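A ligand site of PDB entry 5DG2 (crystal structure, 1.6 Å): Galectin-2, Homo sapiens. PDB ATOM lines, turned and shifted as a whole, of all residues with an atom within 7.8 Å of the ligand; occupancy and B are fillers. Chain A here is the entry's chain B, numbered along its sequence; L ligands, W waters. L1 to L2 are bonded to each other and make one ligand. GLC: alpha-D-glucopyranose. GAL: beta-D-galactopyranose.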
ATOM      1  N   PHE A  34     -13.651   7.500  11.370  1.00  0.00           N
ATOM      2  CA  PHE A  34     -14.064   8.863  11.693  1.00  0.00           C
ATOM      3  C   PHE A  34     -15.162   9.304  10.740  1.00  0.00           C
ATOM      4  O   PHE A  34     -15.474   8.623   9.757  1.00  0.00           O
ATOM      5  CB  PHE A  34     -12.888   9.844  11.652  1.00  0.00           C
ATOM      6  CG  PHE A  34     -12.307  10.067  10.273  1.00  0.00           C
ATOM      7  CD1 PHE A  34     -11.341   9.214   9.778  1.00  0.00           C
ATOM      8  CD2 PHE A  34     -12.720  11.133   9.492  1.00  0.00           C
ATOM      9  CE1 PHE A  34     -10.794   9.425   8.512  1.00  0.00           C
ATOM     10  CE2 PHE A  34     -12.174  11.351   8.239  1.00  0.00           C
ATOM     11  CZ  PHE A  34     -11.214  10.497   7.752  1.00  0.00           C
ATOM     12  N   VAL A  35     -15.723  10.460  11.024  1.00  0.00           N
ATOM     13  CA  VAL A  35     -16.856  10.988  10.271  1.00  0.00           C
ATOM     14  C   VAL A  35     -16.651  12.456   9.903  1.00  0.00           C
ATOM     15  O   VAL A  35     -16.196  13.264  10.718  1.00  0.00           O
ATOM     16  CB  VAL A  35     -18.177  10.871  11.075  1.00  0.00           C
ATOM     17  CG1 VAL A  35     -19.329  11.600  10.368  1.00  0.00           C
ATOM     18  CG2 VAL A  35     -18.555   9.410  11.298  1.00  0.00           C
ATOM     19  N   ASN A  37     -19.293  15.220   8.468  1.00  0.00           N
ATOM     20  CA  ASN A  37     -20.678  15.491   8.099  1.00  0.00           C
ATOM     21  C   ASN A  37     -20.787  16.840   7.448  1.00  0.00           C
ATOM     22  O   ASN A  37     -20.171  17.800   7.899  1.00  0.00           O
ATOM     23  CB  ASN A  37     -21.593  15.448   9.329  1.00  0.00           C
ATOM     24  CG  ASN A  37     -21.773  14.050   9.878  1.00  0.00           C
ATOM     25  OD1 ASN A  37     -21.902  13.083   9.130  1.00  0.00           O
ATOM     26  ND2 ASN A  37     -21.765  13.943  11.206  1.00  0.00           N
ATOM     27  N   HIS A  48     -22.799  12.320   4.698  1.00  0.00           N
ATOM     28  CA  HIS A  48     -22.172  11.691   5.835  1.00  0.00           C
ATOM     29  C   HIS A  48     -21.052  10.842   5.269  1.00  0.00           C
ATOM     30  O   HIS A  48     -21.304   9.853   4.564  1.00  0.00           O
ATOM     31  CB  HIS A  48     -23.200  10.875   6.619  1.00  0.00           C
ATOM     32  CG  HIS A  48     -22.625   9.975   7.660  1.00  0.00           C
ATOM     33  ND1 HIS A  48     -22.207  10.438   8.889  1.00  0.00           N
ATOM     34  CD2 HIS A  48     -22.407   8.638   7.672  1.00  0.00           C
ATOM     35  CE1 HIS A  48     -21.759   9.428   9.615  1.00  0.00           C
ATOM     36  NE2 HIS A  48     -21.862   8.318   8.896  1.00  0.00           N
ATOM     37  N   PHE A  49     -19.822  11.250   5.535  1.00  0.00           N
ATOM     38  CA  PHE A  49     -18.633  10.639   4.949  1.00  0.00           C
ATOM     39  C   PHE A  49     -17.859   9.952   6.067  1.00  0.00           C
ATOM     40  O   PHE A  49     -17.298  10.601   6.946  1.00  0.00           O
ATOM     41  CB  PHE A  49     -17.789  11.711   4.255  1.00  0.00           C
ATOM     42  CG  PHE A  49     -16.446  11.234   3.741  1.00  0.00           C
ATOM     43  CD1 PHE A  49     -16.344  10.522   2.555  1.00  0.00           C
ATOM     44  CD2 PHE A  49     -15.278  11.550   4.443  1.00  0.00           C
ATOM     45  CE1 PHE A  49     -15.096  10.102   2.088  1.00  0.00           C
ATOM     46  CE2 PHE A  49     -14.037  11.152   3.973  1.00  0.00           C
ATOM     47  CZ  PHE A  49     -13.940  10.410   2.793  1.00  0.00           C
ATOM     48  N   ASN A  50     -17.876   8.626   6.038  1.00  0.00           N
ATOM     49  CA  ASN A  50     -17.437   7.845   7.203  1.00  0.00           C
ATOM     50  C   ASN A  50     -16.445   6.741   6.826  1.00  0.00           C
ATOM     51  O   ASN A  50     -16.836   5.594   6.630  1.00  0.00           O
ATOM     52  CB  ASN A  50     -18.687   7.280   7.882  1.00  0.00           C
ATOM     53  CG  ASN A  50     -18.406   6.351   9.059  1.00  0.00           C
ATOM     54  OD1 ASN A  50     -19.270   5.538   9.400  1.00  0.00           O
ATOM     55  ND2 ASN A  50     -17.235   6.459   9.701  1.00  0.00           N
ATOM     56  N   ARG A  52     -14.249   3.876   7.571  1.00  0.00           N
ATOM     57  CA  ARG A  52     -14.280   2.903   8.641  1.00  0.00           C
ATOM     58  C   ARG A  52     -13.094   1.978   8.474  1.00  0.00           C
ATOM     59  O   ARG A  52     -13.196   0.979   7.782  1.00  0.00           O
ATOM     60  CB  ARG A  52     -15.591   2.115   8.625  1.00  0.00           C
ATOM     61  CG  ARG A  52     -16.792   2.971   8.925  1.00  0.00           C
ATOM     62  CD  ARG A  52     -18.019   2.076   9.025  1.00  0.00           C
ATOM     63  NE  ARG A  52     -19.249   2.850   9.127  1.00  0.00           N
ATOM     64  CZ  ARG A  52     -20.460   2.316   9.155  1.00  0.00           C
ATOM     65  NH1 ARG A  52     -20.603   0.996   9.092  1.00  0.00           N
ATOM     66  NH2 ARG A  52     -21.522   3.105   9.237  1.00  0.00           N
ATOM     67  N   GLU A  55     -13.646  -1.616   9.202  1.00  0.00           N
ATOM     68  CA  GLU A  55     -14.382  -2.402   8.196  1.00  0.00           C
ATOM     69  C   GLU A  55     -13.763  -2.290   6.808  1.00  0.00           C
ATOM     70  O   GLU A  55     -14.365  -2.747   5.829  1.00  0.00           O
ATOM     71  CB  GLU A  55     -15.848  -1.953   8.114  1.00  0.00           C
ATOM     72  CG  GLU A  55     -16.652  -2.249   9.350  1.00  0.00           C
ATOM     73  CD  GLU A  55     -18.097  -1.829   9.206  1.00  0.00           C
ATOM     74  OE1 GLU A  55     -18.759  -2.291   8.258  1.00  0.00           O
ATOM     75  OE2 GLU A  55     -18.568  -1.048  10.050  1.00  0.00           O
ATOM     76  N   VAL A  59     -18.032   4.468   4.211  1.00  0.00           N
ATOM     77  CA  VAL A  59     -19.486   4.490   4.140  1.00  0.00           C
ATOM     78  C   VAL A  59     -19.963   5.922   3.912  1.00  0.00           C
ATOM     79  O   VAL A  59     -19.630   6.815   4.681  1.00  0.00           O
ATOM     80  CB  VAL A  59     -20.121   3.919   5.410  1.00  0.00           C
ATOM     81  CG1 VAL A  59     -21.637   4.037   5.354  1.00  0.00           C
ATOM     82  CG2 VAL A  59     -19.706   2.465   5.613  1.00  0.00           C
ATOM     83  N   CYS A  60     -20.719   6.123   2.840  1.00  0.00           N
ATOM     84  CA  CYS A  60     -21.388   7.408   2.599  1.00  0.00           C
ATOM     85  C   CYS A  60     -22.882   7.252   2.756  1.00  0.00           C
ATOM     86  O   CYS A  60     -23.453   6.256   2.324  1.00  0.00           O
ATOM     87  CB  CYS A  60     -21.099   7.937   1.195  1.00  0.00           C
ATOM     88  SG  CYS A  60     -19.399   8.475   0.975  1.00  0.00           S
ATOM     89  N   ASN A  61     -23.516   8.256   3.348  1.00  0.00           N
ATOM     90  CA  ASN A  61     -24.960   8.219   3.469  1.00  0.00           C
ATOM     91  C   ASN A  61     -25.506   9.628   3.630  1.00  0.00           C
ATOM     92  O   ASN A  61     -24.747  10.596   3.735  1.00  0.00           O
ATOM     93  CB  ASN A  61     -25.392   7.357   4.660  1.00  0.00           C
ATOM     94  CG  ASN A  61     -26.745   6.684   4.447  1.00  0.00           C
ATOM     95  OD1 ASN A  61     -27.491   7.062   3.544  1.00  0.00           O
ATOM     96  ND2 ASN A  61     -27.083   5.702   5.277  1.00  0.00           N
ATOM     97  N   SER A  62     -26.817   9.723   3.666  1.00  0.00           N
ATOM     98  CA  SER A  62     -27.520  10.949   3.988  1.00  0.00           C
ATOM     99  C   SER A  62     -28.305  10.720   5.272  1.00  0.00           C
ATOM    100  O   SER A  62     -28.644   9.586   5.588  1.00  0.00           O
ATOM    101  CB  SER A  62     -28.452  11.328   2.840  1.00  0.00           C
ATOM    102  OG  SER A  62     -29.278  10.222   2.514  1.00  0.00           O
ATOM    103  N   LEU A  63     -28.594  11.803   5.988  1.00  0.00           N
ATOM    104  CA  LEU A  63     -29.481  11.718   7.146  1.00  0.00           C
ATOM    105  C   LEU A  63     -30.603  12.723   7.015  1.00  0.00           C
ATOM    106  O   LEU A  63     -30.355  13.922   6.890  1.00  0.00           O
ATOM    107  CB  LEU A  63     -28.719  11.944   8.450  1.00  0.00           C
ATOM    108  CG  LEU A  63     -29.539  11.949   9.733  1.00  0.00           C
ATOM    109  CD1 LEU A  63     -30.131  10.580  10.042  1.00  0.00           C
ATOM    110  CD2 LEU A  63     -28.674  12.448  10.895  1.00  0.00           C
ATOM    111  N   TRP A  68     -31.669   7.523   8.414  1.00  0.00           N
ATOM    112  CA  TRP A  68     -30.547   7.302   7.505  1.00  0.00           C
ATOM    113  C   TRP A  68     -31.057   6.840   6.153  1.00  0.00           C
ATOM    114  O   TRP A  68     -32.056   6.118   6.069  1.00  0.00           O
ATOM    115  CB  TRP A  68     -29.571   6.266   8.078  1.00  0.00           C
ATOM    116  CG  TRP A  68     -28.782   6.776   9.245  1.00  0.00           C
ATOM    117  CD1 TRP A  68     -28.958   6.459  10.559  1.00  0.00           C
ATOM    118  CD2 TRP A  68     -27.708   7.720   9.184  1.00  0.00           C
ATOM    119  NE1 TRP A  68     -28.041   7.144  11.325  1.00  0.00           N
ATOM    120  CE2 TRP A  68     -27.270   7.919  10.514  1.00  0.00           C
ATOM    121  CE3 TRP A  68     -27.070   8.403   8.158  1.00  0.00           C
ATOM    122  CZ2 TRP A  68     -26.222   8.778  10.817  1.00  0.00           C
ATOM    123  CZ3 TRP A  68     -26.033   9.255   8.465  1.00  0.00           C
ATOM    124  CH2 TRP A  68     -25.617   9.432   9.787  1.00  0.00           C
ATOM    125  N   GLY A  69     -30.375   7.265   5.092  1.00  0.00           N
ATOM    126  CA  GLY A  69     -30.725   6.828   3.753  1.00  0.00           C
ATOM    127  C   GLY A  69     -30.083   5.492   3.447  1.00  0.00           C
ATOM    128  O   GLY A  69     -29.651   4.770   4.358  1.00  0.00           O
ATOM    129  N   GLN A  70     -29.998   5.143   2.162  1.00  0.00           N
ATOM    130  CA  GLN A  70     -29.308   3.931   1.755  1.00  0.00           C
ATOM    131  C   GLN A  70     -27.815   4.164   1.695  1.00  0.00           C
ATOM    132  O   GLN A  70     -27.341   5.055   0.984  1.00  0.00           O
ATOM    133  CB  GLN A  70     -29.800   3.428   0.399  1.00  0.00           C
ATOM    134  CG  GLN A  70     -29.171   2.084   0.018  1.00  0.00           C
ATOM    135  CD  GLN A  70     -29.529   1.654  -1.403  1.00  0.00           C
ATOM    136  OE1 GLN A  70     -29.129   2.296  -2.378  1.00  0.00           O
ATOM    137  NE2 GLN A  70     -30.290   0.567  -1.523  1.00  0.00           N
ATOM    138  N   GLU A  71     -27.049   3.356   2.423  1.00  0.00           N
ATOM    139  CA  GLU A  71     -25.594   3.478   2.397  1.00  0.00           C
ATOM    140  C   GLU A  71     -25.006   3.248   1.009  1.00  0.00           C
ATOM    141  O   GLU A  71     -25.519   2.436   0.223  1.00  0.00           O
ATOM    142  CB  GLU A  71     -24.949   2.488   3.366  1.00  0.00           C
ATOM    143  CG  GLU A  71     -25.197   2.853   4.805  1.00  0.00           C
ATOM    144  CD  GLU A  71     -24.577   1.881   5.796  1.00  0.00           C
ATOM    145  OE1 GLU A  71     -24.650   2.173   7.005  1.00  0.00           O
ATOM    146  OE2 GLU A  71     -24.042   0.835   5.389  1.00  0.00           O
ATOM    147  N   GLN A  72     -23.934   3.984   0.732  1.00  0.00           N
ATOM    148  CA  GLN A  72     -23.112   3.748  -0.438  1.00  0.00           C
ATOM    149  C   GLN A  72     -21.703   3.452   0.061  1.00  0.00           C
ATOM    150  O   GLN A  72     -21.085   4.318   0.680  1.00  0.00           O
ATOM    151  CB  GLN A  72     -23.134   4.949  -1.382  1.00  0.00           C
ATOM    152  CG  GLN A  72     -22.337   4.759  -2.667  1.00  0.00           C
ATOM    153  CD  GLN A  72     -22.436   5.963  -3.594  1.00  0.00           C
ATOM    154  OE1 GLN A  72     -23.521   6.425  -3.925  1.00  0.00           O
ATOM    155  NE2 GLN A  72     -21.287   6.466  -4.017  1.00  0.00           N
ATOM    156  N   ARG A  73     -21.224   2.237  -0.154  1.00  0.00           N
ATOM    157  CA  ARG A  73     -19.929   1.826   0.383  1.00  0.00           C
ATOM    158  C   ARG A  73     -18.879   1.776  -0.703  1.00  0.00           C
ATOM    159  O   ARG A  73     -19.122   1.257  -1.803  1.00  0.00           O
ATOM    160  CB  ARG A  73     -20.030   0.459   1.085  1.00  0.00           C
ATOM    161  CG  ARG A  73     -20.956   0.455   2.273  1.00  0.00           C
ATOM    162  CD  ARG A  73     -20.653  -0.681   3.227  1.00  0.00           C
ATOM    163  NE  ARG A  73     -21.495  -0.576   4.416  1.00  0.00           N
ATOM    164  CZ  ARG A  73     -21.169  -1.064   5.603  1.00  0.00           C
ATOM    165  NH1 ARG A  73     -20.013  -1.702   5.777  1.00  0.00           N
ATOM    166  NH2 ARG A  73     -21.999  -0.908   6.630  1.00  0.00           N
ATOM    167  N   ARG A 123     -16.575  13.707  13.743  1.00  0.00           N
ATOM    168  CA  ARG A 123     -16.725  12.804  14.868  1.00  0.00           C
ATOM    169  C   ARG A 123     -15.638  11.741  14.774  1.00  0.00           C
ATOM    170  O   ARG A 123     -15.130  11.445  13.684  1.00  0.00           O
ATOM    171  CB  ARG A 123     -18.099  12.126  14.867  1.00  0.00           C
ATOM    172  CG  ARG A 123     -19.295  13.069  14.761  1.00  0.00           C
ATOM    173  CD  ARG A 123     -19.570  13.750  16.076  1.00  0.00           C
ATOM    174  NE  ARG A 123     -20.755  14.618  16.021  1.00  0.00           N
ATOM    175  CZ  ARG A 123     -20.707  15.949  16.011  1.00  0.00           C
ATOM    176  NH1 ARG A 123     -19.542  16.582  16.036  1.00  0.00           N
ATOM    177  NH2 ARG A 123     -21.841  16.640  15.962  1.00  0.00           N
HETATM  178  C1  GLC L   1     -26.628  -0.812   9.646  1.00  0.00           C
HETATM  179  C2  GLC L   1     -25.239  -0.523   9.017  1.00  0.00           C
HETATM  180  C3  GLC L   1     -24.304   0.241   9.857  1.00  0.00           C
HETATM  181  C4  GLC L   1     -24.999   1.216  10.677  1.00  0.00           C
HETATM  182  C5  GLC L   1     -25.799   0.513  11.704  1.00  0.00           C
HETATM  183  C6  GLC L   1     -26.560   1.511  12.564  1.00  0.00           C
HETATM  184  O1  GLC L   1     -27.034  -2.026   9.419  1.00  0.00           O
HETATM  185  O2  GLC L   1     -24.596  -1.754   8.647  1.00  0.00           O
HETATM  186  O3  GLC L   1     -23.381   0.926   8.925  1.00  0.00           O
HETATM  187  O4  GLC L   1     -24.009   2.111  11.360  1.00  0.00           O
HETATM  188  O5  GLC L   1     -26.781  -0.419  11.125  1.00  0.00           O
HETATM  189  O6  GLC L   1     -27.615   2.024  11.768  1.00  0.00           O
HETATM  190  C1  GAL L   2     -24.436   3.427  11.258  1.00  0.00           C
HETATM  191  C2  GAL L   2     -23.595   4.333  12.145  1.00  0.00           C
HETATM  192  C3  GAL L   2     -23.751   5.783  11.850  1.00  0.00           C
HETATM  193  C4  GAL L   2     -23.719   6.080  10.397  1.00  0.00           C
HETATM  194  C5  GAL L   2     -24.645   5.215   9.564  1.00  0.00           C
HETATM  195  C6  GAL L   2     -24.499   5.426   8.088  1.00  0.00           C
HETATM  196  O2  GAL L   2     -23.836   4.089  13.569  1.00  0.00           O
HETATM  197  O3  GAL L   2     -22.711   6.515  12.539  1.00  0.00           O
HETATM  198  O4  GAL L   2     -22.351   5.883   9.935  1.00  0.00           O
HETATM  199  O5  GAL L   2     -24.378   3.778   9.845  1.00  0.00           O
HETATM  200  O6  GAL L   2     -25.470   4.674   7.412  1.00  0.00           O
HETATM  201  O   HOH W   1     -28.640   4.349  13.787  1.00  0.00           O
HETATM  202  O   HOH W   2     -21.319  -2.203   9.472  1.00  0.00           O
HETATM  203  O   HOH W   3     -22.455   9.186  13.101  1.00  0.00           O
HETATM  204  O   HOH W   4     -20.256   5.676  11.969  1.00  0.00           O
HETATM  205  O   HOH W   5     -27.654   3.153   8.641  1.00  0.00           O
HETATM  206  O   HOH W   6     -22.568   6.142  15.440  1.00  0.00           O
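Water W4 bridges an oxygen (O3) of GAL L2 and the side-chain amide oxygen of Asn 50. Water W2 lies within hydrogen-bond range of the side-chain carboxylate of Glu 55 (2.8 Å), the guanidinium group of Arg 73 (3.2 Å), the guanidinium group of Arg 52 (3.3 Å) and an oxygen (O2) of GLC L1 (3.4 Å).
CZ2 of Trp 68 touches C4 of GAL L2, at 3.7 Å. Hydrophobic or aromatic side chains that line the ligand: His 48 and Trp 68. Within 4 Å of the ligand: His 48, Asn 50, Arg 52, Asn 61, Trp 68, Glu 71 and Arg 73.
NH2 of Arg 52 is in salt-bridge range of OE1 of Glu 71, at 3.95 Å. The guanidinium group of Arg 73 is in salt-bridge range of the side-chain carboxylate of Glu 71 (3.0 Å). A ring nitrogen (ND1) of His 48 is in hydrogen-bond range of the side-chain amide oxygen (OD1) of Asn 37 (2.7 Å). OD1 of Asn 50 lies within hydrogen-bond range of NE of Arg 52 (2.7 Å). The side-chain amide nitrogen (ND2) of Asn 61 sits at hydrogen-bond distance from the backbone carbonyl oxygen (O) of Gly 69, 2.9 Å away. The backbone carbonyl oxygen of Val 59 lies within hydrogen-bond range of the backbone NH of Asn 50, 2.9 Å away. The side-chain amide nitrogen (ND2) of Asn 50 sits at hydrogen-bond distance from the backbone carbonyl oxygen (O) of Phe 34, 2.8 Å away. The guanidinium group of Arg 73 is in salt-bridge range of the side-chain carboxylate of Glu 55, at 2.8 Å.
O3 of GLC L1 sits at hydrogen-bond distance from OE1 of Glu 71 (2.6 Å). A ring nitrogen (NE2) of His 48 is in hydrogen-bond range of an oxygen (O4) of GAL L2. An oxygen (O3) of GLC L1 sits at hydrogen-bond distance from the guanidinium group (NH1) of Arg 52 (2.8 Å). The side-chain amide nitrogen (ND2) of Asn 61 sits at hydrogen-bond distance from an oxygen (O6) of GAL L2 (2.9 Å). OD1 of Asn 50 is in hydrogen-bond range of O4 of GAL L2, 3.1 Å away. The guanidinium group (NH2) of Arg 73 is in hydrogen-bond range of an oxygen (O3) of GLC L1.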
